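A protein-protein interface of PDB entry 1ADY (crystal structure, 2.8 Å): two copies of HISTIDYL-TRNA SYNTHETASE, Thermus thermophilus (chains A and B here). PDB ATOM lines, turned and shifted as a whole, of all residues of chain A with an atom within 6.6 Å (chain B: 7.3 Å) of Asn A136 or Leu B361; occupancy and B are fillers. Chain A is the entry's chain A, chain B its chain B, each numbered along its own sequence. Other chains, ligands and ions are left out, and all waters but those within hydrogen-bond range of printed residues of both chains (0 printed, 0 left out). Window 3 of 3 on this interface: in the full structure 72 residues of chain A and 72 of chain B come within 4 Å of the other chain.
O of Gln A100 lies within hydrogen-bond range of NH2 of Arg B376 (3.4 Å). ND2 of Asn A136 sits at hydrogen-bond distance from O of Leu B361 (3.3 Å).
The backbone NH (N) of Ile A138 lies within hydrogen-bond range of the side-chain amide oxygen (OD1) of Asn A136. The guanidinium group of Arg A287 is in hydrogen-bond range of the backbone carbonyl oxygen of Ser A134 (3.0 Å). The side-chain hydroxyl (OG) of Ser A134 sits at hydrogen-bond distance from the backbone NH (N) of Asn A136.
NH2 of Arg A103 touches OH of Tyr B359 (3.7 Å). Leu B361 touches Ser A134. Ile A138 touches Phe B345. CG2 of Ile A138 touches OH of Tyr B359, at 3.6 Å. Ile A138 touches Leu B361 (CD1 to CD2, 3.7 Å). Leu A139 touches Leu B361.
Printed residues of chain B within 4 Å of Arg A103: Tyr B359 (3.7 Å). Printed residues of chain B within 4 Å of Asn A136: Leu B361. Printed residues of chain A within 4 Å of Tyr B359: Arg A103 and Ile A138. Of chain A, only Ser A134 (3.7 Å), Asn A136 (3.3 Å), Ile A138 (3.7 Å) and Leu A139 (3.6 Å) come within 4 Å of Leu B361. Of the printed residues of chain A, Arg B376 touches Gln A100 (3.4 Å). The nearest residue of chain B that does not touch Asn A136 is Val B341 (5.4 Å).
Printed residues of chain B that touch a printed residue of chain A: Phe B345, Tyr B359, Leu B361 and Arg B376. Hydrophobic or aromatic side chains of chain A that line the printed part of chain B: Ile A138 and Leu A139. Among the printed residues, 8 pairs touch across the chains.
No position is printed for both chains.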
ATOM      1  N   GLN A 100      14.041  13.876 -22.353  1.00  0.00           N
ATOM      2  CA  GLN A 100      12.613  13.755 -22.632  1.00  0.00           C
ATOM      3  C   GLN A 100      11.844  14.957 -22.090  1.00  0.00           C
ATOM      4  O   GLN A 100      12.269  15.581 -21.114  1.00  0.00           O
ATOM      5  CB  GLN A 100      12.065  12.473 -22.002  1.00  0.00           C
ATOM      6  CG  GLN A 100      12.823  11.213 -22.383  1.00  0.00           C
ATOM      7  CD  GLN A 100      12.748  10.912 -23.859  1.00  0.00           C
ATOM      8  OE1 GLN A 100      11.677  10.976 -24.466  1.00  0.00           O
ATOM      9  NE2 GLN A 100      13.888  10.594 -24.454  1.00  0.00           N
ATOM     10  N   PRO A 101      10.708  15.306 -22.721  1.00  0.00           N
ATOM     11  CA  PRO A 101      10.156  14.618 -23.893  1.00  0.00           C
ATOM     12  C   PRO A 101      10.809  15.102 -25.187  1.00  0.00           C
ATOM     13  O   PRO A 101      11.331  16.219 -25.253  1.00  0.00           O
ATOM     14  CB  PRO A 101       8.678  15.000 -23.836  1.00  0.00           C
ATOM     15  CG  PRO A 101       8.720  16.394 -23.305  1.00  0.00           C
ATOM     16  CD  PRO A 101       9.758  16.310 -22.203  1.00  0.00           C
ATOM     17  N   ARG A 103      10.306  16.404 -28.713  1.00  0.00           N
ATOM     18  CA  ARG A 103       9.320  17.032 -29.600  1.00  0.00           C
ATOM     19  C   ARG A 103       9.865  17.113 -31.033  1.00  0.00           C
ATOM     20  O   ARG A 103      10.976  17.610 -31.258  1.00  0.00           O
ATOM     21  CB  ARG A 103       8.958  18.431 -29.091  1.00  0.00           C
ATOM     22  CG  ARG A 103       8.248  18.446 -27.744  1.00  0.00           C
ATOM     23  CD  ARG A 103       8.023  19.867 -27.254  1.00  0.00           C
ATOM     24  NE  ARG A 103       7.263  19.935 -26.002  1.00  0.00           N
ATOM     25  CZ  ARG A 103       7.776  19.733 -24.788  1.00  0.00           C
ATOM     26  NH1 ARG A 103       9.061  19.438 -24.632  1.00  0.00           N
ATOM     27  NH2 ARG A 103       7.002  19.848 -23.719  1.00  0.00           N
ATOM     28  N   SER A 134       6.663  10.648 -22.802  1.00  0.00           N
ATOM     29  CA  SER A 134       5.971  10.951 -21.549  1.00  0.00           C
ATOM     30  C   SER A 134       4.451  10.807 -21.597  1.00  0.00           C
ATOM     31  O   SER A 134       3.811  11.086 -22.613  1.00  0.00           O
ATOM     32  CB  SER A 134       6.341  12.356 -21.066  1.00  0.00           C
ATOM     33  OG  SER A 134       5.699  12.667 -19.840  1.00  0.00           O
ATOM     34  N   GLU A 135       3.891  10.386 -20.469  1.00  0.00           N
ATOM     35  CA  GLU A 135       2.457  10.174 -20.315  1.00  0.00           C
ATOM     36  C   GLU A 135       1.777  11.409 -19.719  1.00  0.00           C
ATOM     37  O   GLU A 135       0.548  11.546 -19.775  1.00  0.00           O
ATOM     38  CB  GLU A 135       2.233   8.955 -19.412  1.00  0.00           C
ATOM     39  CG  GLU A 135       0.794   8.668 -19.038  1.00  0.00           C
ATOM     40  CD  GLU A 135      -0.007   8.102 -20.178  1.00  0.00           C
ATOM     41  OE1 GLU A 135       0.119   6.887 -20.434  1.00  0.00           O
ATOM     42  OE2 GLU A 135      -0.766   8.868 -20.808  1.00  0.00           O
ATOM     43  N   ASN A 136       2.582  12.319 -19.182  1.00  0.00           N
ATOM     44  CA  ASN A 136       2.076  13.535 -18.552  1.00  0.00           C
ATOM     45  C   ASN A 136       1.061  14.280 -19.414  1.00  0.00           C
ATOM     46  O   ASN A 136       1.389  14.769 -20.497  1.00  0.00           O
ATOM     47  CB  ASN A 136       3.233  14.463 -18.197  1.00  0.00           C
ATOM     48  CG  ASN A 136       2.806  15.610 -17.312  1.00  0.00           C
ATOM     49  OD1 ASN A 136       1.777  16.243 -17.550  1.00  0.00           O
ATOM     50  ND2 ASN A 136       3.588  15.881 -16.272  1.00  0.00           N
ATOM     51  N   PRO A 137      -0.177  14.414 -18.919  1.00  0.00           N
ATOM     52  CA  PRO A 137      -1.279  15.097 -19.610  1.00  0.00           C
ATOM     53  C   PRO A 137      -1.015  16.543 -20.028  1.00  0.00           C
ATOM     54  O   PRO A 137      -1.803  17.118 -20.779  1.00  0.00           O
ATOM     55  CB  PRO A 137      -2.430  14.992 -18.606  1.00  0.00           C
ATOM     56  CG  PRO A 137      -1.718  14.911 -17.278  1.00  0.00           C
ATOM     57  CD  PRO A 137      -0.606  13.953 -17.588  1.00  0.00           C
ATOM     58  N   ILE A 138       0.078  17.134 -19.548  1.00  0.00           N
ATOM     59  CA  ILE A 138       0.423  18.512 -19.905  1.00  0.00           C
ATOM     60  C   ILE A 138       0.732  18.590 -21.402  1.00  0.00           C
ATOM     61  O   ILE A 138       0.304  19.520 -22.094  1.00  0.00           O
ATOM     62  CB  ILE A 138       1.635  19.027 -19.093  1.00  0.00           C
ATOM     63  CG1 ILE A 138       1.241  19.217 -17.626  1.00  0.00           C
ATOM     64  CG2 ILE A 138       2.150  20.339 -19.681  1.00  0.00           C
ATOM     65  CD1 ILE A 138       2.375  19.678 -16.727  1.00  0.00           C
ATOM     66  N   LEU A 139       1.435  17.572 -21.894  1.00  0.00           N
ATOM     67  CA  LEU A 139       1.811  17.479 -23.296  1.00  0.00           C
ATOM     68  C   LEU A 139       0.575  17.390 -24.184  1.00  0.00           C
ATOM     69  O   LEU A 139       0.545  17.949 -25.278  1.00  0.00           O
ATOM     70  CB  LEU A 139       2.698  16.258 -23.507  1.00  0.00           C
ATOM     71  CG  LEU A 139       3.975  16.260 -22.670  1.00  0.00           C
ATOM     72  CD1 LEU A 139       4.766  14.994 -22.928  1.00  0.00           C
ATOM     73  CD2 LEU A 139       4.804  17.477 -23.011  1.00  0.00           C
ATOM     74  N   ASP A 140      -0.451  16.706 -23.689  1.00  0.00           N
ATOM     75  CA  ASP A 140      -1.701  16.550 -24.420  1.00  0.00           C
ATOM     76  C   ASP A 140      -2.357  17.922 -24.557  1.00  0.00           C
ATOM     77  O   ASP A 140      -2.839  18.293 -25.633  1.00  0.00           O
ATOM     78  CB  ASP A 140      -2.645  15.592 -23.679  1.00  0.00           C
ATOM     79  CG  ASP A 140      -2.048  14.205 -23.488  1.00  0.00           C
ATOM     80  OD1 ASP A 140      -1.008  14.081 -22.809  1.00  0.00           O
ATOM     81  OD2 ASP A 140      -2.635  13.240 -24.011  1.00  0.00           O
ATOM     82  N   ALA A 141      -2.373  18.678 -23.461  1.00  0.00           N
ATOM     83  CA  ALA A 141      -2.956  20.014 -23.461  1.00  0.00           C
ATOM     84  C   ALA A 141      -2.140  20.881 -24.416  1.00  0.00           C
ATOM     85  O   ALA A 141      -2.697  21.561 -25.279  1.00  0.00           O
ATOM     86  CB  ALA A 141      -2.933  20.603 -22.059  1.00  0.00           C
ATOM     87  N   HIS A 236      -6.915  11.356 -16.364  1.00  0.00           N
ATOM     88  CA  HIS A 236      -6.012  11.960 -17.338  1.00  0.00           C
ATOM     89  C   HIS A 236      -6.739  13.016 -18.170  1.00  0.00           C
ATOM     90  O   HIS A 236      -6.255  14.139 -18.321  1.00  0.00           O
ATOM     91  CB  HIS A 236      -5.447  10.861 -18.250  1.00  0.00           C
ATOM     92  CG  HIS A 236      -4.243  11.273 -19.038  1.00  0.00           C
ATOM     93  ND1 HIS A 236      -4.331  11.882 -20.273  1.00  0.00           N
ATOM     94  CD2 HIS A 236      -2.922  11.124 -18.784  1.00  0.00           C
ATOM     95  CE1 HIS A 236      -3.114  12.087 -20.744  1.00  0.00           C
ATOM     96  NE2 HIS A 236      -2.241  11.637 -19.860  1.00  0.00           N
ATOM     97  N   HIS A 243      -6.082  22.032 -17.780  1.00  0.00           N
ATOM     98  CA  HIS A 243      -5.055  22.844 -18.419  1.00  0.00           C
ATOM     99  C   HIS A 243      -5.627  23.728 -19.522  1.00  0.00           C
ATOM    100  O   HIS A 243      -5.331  24.921 -19.574  1.00  0.00           O
ATOM    101  CB  HIS A 243      -3.960  21.954 -18.991  1.00  0.00           C
ATOM    102  CG  HIS A 243      -3.239  21.144 -17.962  1.00  0.00           C
ATOM    103  ND1 HIS A 243      -2.889  21.648 -16.728  1.00  0.00           N
ATOM    104  CD2 HIS A 243      -2.777  19.870 -17.995  1.00  0.00           C
ATOM    105  CE1 HIS A 243      -2.243  20.720 -16.044  1.00  0.00           C
ATOM    106  NE2 HIS A 243      -2.162  19.632 -16.790  1.00  0.00           N
ATOM    107  N   ARG A 287      -3.310  11.041 -28.315  1.00  0.00           N
ATOM    108  CA  ARG A 287      -2.257  10.251 -27.700  1.00  0.00           C
ATOM    109  C   ARG A 287      -2.235   8.891 -28.386  1.00  0.00           C
ATOM    110  O   ARG A 287      -3.260   8.441 -28.904  1.00  0.00           O
ATOM    111  CB  ARG A 287      -2.520  10.128 -26.202  1.00  0.00           C
ATOM    112  CG  ARG A 287      -1.451   9.398 -25.423  1.00  0.00           C
ATOM    113  CD  ARG A 287      -1.532   9.727 -23.943  1.00  0.00           C
ATOM    114  NE  ARG A 287      -0.843  10.976 -23.608  1.00  0.00           N
ATOM    115  CZ  ARG A 287       0.476  11.083 -23.464  1.00  0.00           C
ATOM    116  NH1 ARG A 287       1.254  10.016 -23.627  1.00  0.00           N
ATOM    117  NH2 ARG A 287       1.021  12.247 -23.125  1.00  0.00           N
ATOM    118  N   PRO A 301       5.430   6.598 -24.682  1.00  0.00           N
ATOM    119  CA  PRO A 301       4.184   7.369 -24.722  1.00  0.00           C
ATOM    120  C   PRO A 301       4.351   8.546 -25.680  1.00  0.00           C
ATOM    121  O   PRO A 301       5.473   9.021 -25.887  1.00  0.00           O
ATOM    122  CB  PRO A 301       4.038   7.857 -23.278  1.00  0.00           C
ATOM    123  CG  PRO A 301       4.843   6.853 -22.474  1.00  0.00           C
ATOM    124  CD  PRO A 301       6.041   6.640 -23.342  1.00  0.00           C
ATOM    125  N   VAL A 303       2.061  12.060 -27.847  1.00  0.00           N
ATOM    126  CA  VAL A 303       0.891  12.826 -28.266  1.00  0.00           C
ATOM    127  C   VAL A 303       1.325  13.702 -29.433  1.00  0.00           C
ATOM    128  O   VAL A 303       2.512  13.998 -29.590  1.00  0.00           O
ATOM    129  CB  VAL A 303       0.377  13.792 -27.168  1.00  0.00           C
ATOM    130  CG1 VAL A 303      -1.091  13.547 -26.899  1.00  0.00           C
ATOM    131  CG2 VAL A 303       1.205  13.689 -25.907  1.00  0.00           C
ATOM    132  N   TYR B 332      14.486  28.072 -19.752  1.00  0.00           N
ATOM    133  CA  TYR B 332      14.113  26.719 -19.367  1.00  0.00           C
ATOM    134  C   TYR B 332      13.604  26.812 -17.938  1.00  0.00           C
ATOM    135  O   TYR B 332      14.372  27.091 -17.012  1.00  0.00           O
ATOM    136  CB  TYR B 332      15.309  25.765 -19.433  1.00  0.00           C
ATOM    137  CG  TYR B 332      14.950  24.339 -19.070  1.00  0.00           C
ATOM    138  CD1 TYR B 332      14.134  23.574 -19.904  1.00  0.00           C
ATOM    139  CD2 TYR B 332      15.415  23.759 -17.887  1.00  0.00           C
ATOM    140  CE1 TYR B 332      13.785  22.269 -19.571  1.00  0.00           C
ATOM    141  CE2 TYR B 332      15.075  22.452 -17.544  1.00  0.00           C
ATOM    142  CZ  TYR B 332      14.259  21.713 -18.390  1.00  0.00           C
ATOM    143  OH  TYR B 332      13.920  20.419 -18.058  1.00  0.00           O
ATOM    144  N   LEU B 333      12.299  26.635 -17.774  1.00  0.00           N
ATOM    145  CA  LEU B 333      11.671  26.702 -16.463  1.00  0.00           C
ATOM    146  C   LEU B 333      11.777  25.378 -15.722  1.00  0.00           C
ATOM    147  O   LEU B 333      11.463  24.313 -16.265  1.00  0.00           O
ATOM    148  CB  LEU B 333      10.208  27.121 -16.597  1.00  0.00           C
ATOM    149  CG  LEU B 333       9.993  28.543 -17.112  1.00  0.00           C
ATOM    150  CD1 LEU B 333       8.537  28.780 -17.451  1.00  0.00           C
ATOM    151  CD2 LEU B 333      10.480  29.540 -16.076  1.00  0.00           C
ATOM    152  N   PRO B 335      10.497  23.493 -12.306  1.00  0.00           N
ATOM    153  CA  PRO B 335       9.542  23.473 -11.192  1.00  0.00           C
ATOM    154  C   PRO B 335      10.176  22.859  -9.949  1.00  0.00           C
ATOM    155  O   PRO B 335      10.816  21.802 -10.023  1.00  0.00           O
ATOM    156  CB  PRO B 335       8.420  22.567 -11.715  1.00  0.00           C
ATOM    157  CG  PRO B 335       8.609  22.555 -13.207  1.00  0.00           C
ATOM    158  CD  PRO B 335      10.099  22.516 -13.331  1.00  0.00           C
ATOM    159  N   GLU B 338       5.305  20.230  -7.205  1.00  0.00           N
ATOM    160  CA  GLU B 338       4.404  19.625  -8.184  1.00  0.00           C
ATOM    161  C   GLU B 338       3.422  20.640  -8.774  1.00  0.00           C
ATOM    162  O   GLU B 338       3.107  20.591  -9.959  1.00  0.00           O
ATOM    163  CB  GLU B 338       3.649  18.447  -7.567  1.00  0.00           C
ATOM    164  CG  GLU B 338       2.962  17.528  -8.580  1.00  0.00           C
ATOM    165  CD  GLU B 338       3.943  16.777  -9.473  1.00  0.00           C
ATOM    166  OE1 GLU B 338       4.779  16.009  -8.945  1.00  0.00           O
ATOM    167  OE2 GLU B 338       3.870  16.951 -10.708  1.00  0.00           O
ATOM    168  N   VAL B 341       4.920  22.698 -11.824  1.00  0.00           N
ATOM    169  CA  VAL B 341       5.033  22.167 -13.183  1.00  0.00           C
ATOM    170  C   VAL B 341       3.972  22.755 -14.108  1.00  0.00           C
ATOM    171  O   VAL B 341       4.301  23.300 -15.160  1.00  0.00           O
ATOM    172  CB  VAL B 341       5.004  20.601 -13.241  1.00  0.00           C
ATOM    173  CG1 VAL B 341       6.038  20.013 -12.299  1.00  0.00           C
ATOM    174  CG2 VAL B 341       3.624  20.061 -12.917  1.00  0.00           C
ATOM    175  N   ALA B 342       2.716  22.727 -13.677  1.00  0.00           N
ATOM    176  CA  ALA B 342       1.636  23.255 -14.497  1.00  0.00           C
ATOM    177  C   ALA B 342       1.814  24.747 -14.702  1.00  0.00           C
ATOM    178  O   ALA B 342       1.573  25.263 -15.790  1.00  0.00           O
ATOM    179  CB  ALA B 342       0.289  22.963 -13.858  1.00  0.00           C
ATOM    180  N   PHE B 345       4.366  25.541 -17.359  1.00  0.00           N
ATOM    181  CA  PHE B 345       3.748  25.369 -18.664  1.00  0.00           C
ATOM    182  C   PHE B 345       2.983  26.635 -19.049  1.00  0.00           C
ATOM    183  O   PHE B 345       3.178  27.183 -20.137  1.00  0.00           O
ATOM    184  CB  PHE B 345       2.814  24.153 -18.625  1.00  0.00           C
ATOM    185  CG  PHE B 345       1.901  24.033 -19.815  1.00  0.00           C
ATOM    186  CD1 PHE B 345       2.410  23.997 -21.110  1.00  0.00           C
ATOM    187  CD2 PHE B 345       0.521  23.945 -19.636  1.00  0.00           C
ATOM    188  CE1 PHE B 345       1.560  23.873 -22.212  1.00  0.00           C
ATOM    189  CE2 PHE B 345      -0.334  23.820 -20.728  1.00  0.00           C
ATOM    190  CZ  PHE B 345       0.191  23.785 -22.021  1.00  0.00           C
ATOM    191  N   TYR B 359      10.304  23.743 -20.479  1.00  0.00           N
ATOM    192  CA  TYR B 359      10.152  23.467 -19.057  1.00  0.00           C
ATOM    193  C   TYR B 359      10.227  21.971 -18.758  1.00  0.00           C
ATOM    194  O   TYR B 359      10.051  21.137 -19.656  1.00  0.00           O
ATOM    195  CB  TYR B 359       8.798  24.007 -18.592  1.00  0.00           C
ATOM    196  CG  TYR B 359       7.646  23.480 -19.424  1.00  0.00           C
ATOM    197  CD1 TYR B 359       7.086  22.228 -19.159  1.00  0.00           C
ATOM    198  CD2 TYR B 359       7.155  24.203 -20.513  1.00  0.00           C
ATOM    199  CE1 TYR B 359       6.076  21.707 -19.957  1.00  0.00           C
ATOM    200  CE2 TYR B 359       6.142  23.690 -21.318  1.00  0.00           C
ATOM    201  CZ  TYR B 359       5.607  22.441 -21.035  1.00  0.00           C
ATOM    202  OH  TYR B 359       4.605  21.916 -21.820  1.00  0.00           O
ATOM    203  N   ALA B 360      10.466  21.639 -17.491  1.00  0.00           N
ATOM    204  CA  ALA B 360      10.536  20.248 -17.048  1.00  0.00           C
ATOM    205  C   ALA B 360       9.131  19.791 -16.658  1.00  0.00           C
ATOM    206  O   ALA B 360       8.313  20.596 -16.215  1.00  0.00           O
ATOM    207  CB  ALA B 360      11.476  20.125 -15.871  1.00  0.00           C
ATOM    208  N   LEU B 361       8.841  18.505 -16.832  1.00  0.00           N
ATOM    209  CA  LEU B 361       7.517  17.978 -16.499  1.00  0.00           C
ATOM    210  C   LEU B 361       7.431  17.343 -15.118  1.00  0.00           C
ATOM    211  O   LEU B 361       6.466  16.633 -14.813  1.00  0.00           O
ATOM    212  CB  LEU B 361       7.052  16.968 -17.550  1.00  0.00           C
ATOM    213  CG  LEU B 361       6.460  17.508 -18.852  1.00  0.00           C
ATOM    214  CD1 LEU B 361       5.938  16.329 -19.660  1.00  0.00           C
ATOM    215  CD2 LEU B 361       5.335  18.499 -18.570  1.00  0.00           C
ATOM    216  N   ALA B 362       8.422  17.617 -14.278  1.00  0.00           N
ATOM    217  CA  ALA B 362       8.468  17.061 -12.932  1.00  0.00           C
ATOM    218  C   ALA B 362       9.311  17.959 -12.040  1.00  0.00           C
ATOM    219  O   ALA B 362      10.208  18.653 -12.517  1.00  0.00           O
ATOM    220  CB  ALA B 362       9.060  15.655 -12.967  1.00  0.00           C
ATOM    221  N   PRO B 363       8.997  17.999 -10.738  1.00  0.00           N
ATOM    222  CA  PRO B 363       9.749  18.828  -9.793  1.00  0.00           C
ATOM    223  C   PRO B 363      11.143  18.243  -9.581  1.00  0.00           C
ATOM    224  O   PRO B 363      11.330  17.026  -9.662  1.00  0.00           O
ATOM    225  CB  PRO B 363       8.916  18.725  -8.513  1.00  0.00           C
ATOM    226  CG  PRO B 363       7.542  18.403  -9.011  1.00  0.00           C
ATOM    227  CD  PRO B 363       7.820  17.406 -10.083  1.00  0.00           C
ATOM    228  N   ARG B 364      12.116  19.102  -9.311  1.00  0.00           N
ATOM    229  CA  ARG B 364      13.481  18.650  -9.082  1.00  0.00           C
ATOM    230  C   ARG B 364      14.283  19.693  -8.318  1.00  0.00           C
ATOM    231  O   ARG B 364      13.886  20.856  -8.237  1.00  0.00           O
ATOM    232  CB  ARG B 364      14.172  18.315 -10.414  1.00  0.00           C
ATOM    233  CG  ARG B 364      14.220  19.460 -11.428  1.00  0.00           C
ATOM    234  CD  ARG B 364      13.486  19.092 -12.718  1.00  0.00           C
ATOM    235  NE  ARG B 364      13.967  17.829 -13.278  1.00  0.00           N
ATOM    236  CZ  ARG B 364      13.226  16.992 -14.003  1.00  0.00           C
ATOM    237  NH1 ARG B 364      11.957  17.269 -14.278  1.00  0.00           N
ATOM    238  NH2 ARG B 364      13.746  15.850 -14.421  1.00  0.00           N
ATOM    239  N   GLU B 372      20.158  20.449 -16.245  1.00  0.00           N
ATOM    240  CA  GLU B 372      19.374  20.201 -17.455  1.00  0.00           C
ATOM    241  C   GLU B 372      19.261  21.420 -18.355  1.00  0.00           C
ATOM    242  O   GLU B 372      19.236  21.295 -19.577  1.00  0.00           O
ATOM    243  CB  GLU B 372      17.983  19.709 -17.086  1.00  0.00           C
ATOM    244  CG  GLU B 372      17.980  18.333 -16.465  1.00  0.00           C
ATOM    245  CD  GLU B 372      16.618  17.913 -15.964  1.00  0.00           C
ATOM    246  OE1 GLU B 372      15.646  18.692 -16.111  1.00  0.00           O
ATOM    247  OE2 GLU B 372      16.526  16.798 -15.412  1.00  0.00           O
ATOM    248  N   ARG B 376      20.602  21.610 -22.150  1.00  0.00           N
ATOM    249  CA  ARG B 376      19.761  21.987 -23.283  1.00  0.00           C
ATOM    250  C   ARG B 376      20.253  23.271 -23.941  1.00  0.00           C
ATOM    251  O   ARG B 376      19.611  23.786 -24.857  1.00  0.00           O
ATOM    252  CB  ARG B 376      18.325  22.210 -22.820  1.00  0.00           C
ATOM    253  CG  ARG B 376      17.525  20.956 -22.556  1.00  0.00           C
ATOM    254  CD  ARG B 376      16.128  21.335 -22.097  1.00  0.00           C
ATOM    255  NE  ARG B 376      15.191  20.219 -22.144  1.00  0.00           N
ATOM    256  CZ  ARG B 376      15.270  19.132 -21.383  1.00  0.00           C
ATOM    257  NH1 ARG B 376      16.251  19.000 -20.499  1.00  0.00           N
ATOM    258  NH2 ARG B 376      14.359  18.176 -21.507  1.00  0.00           N
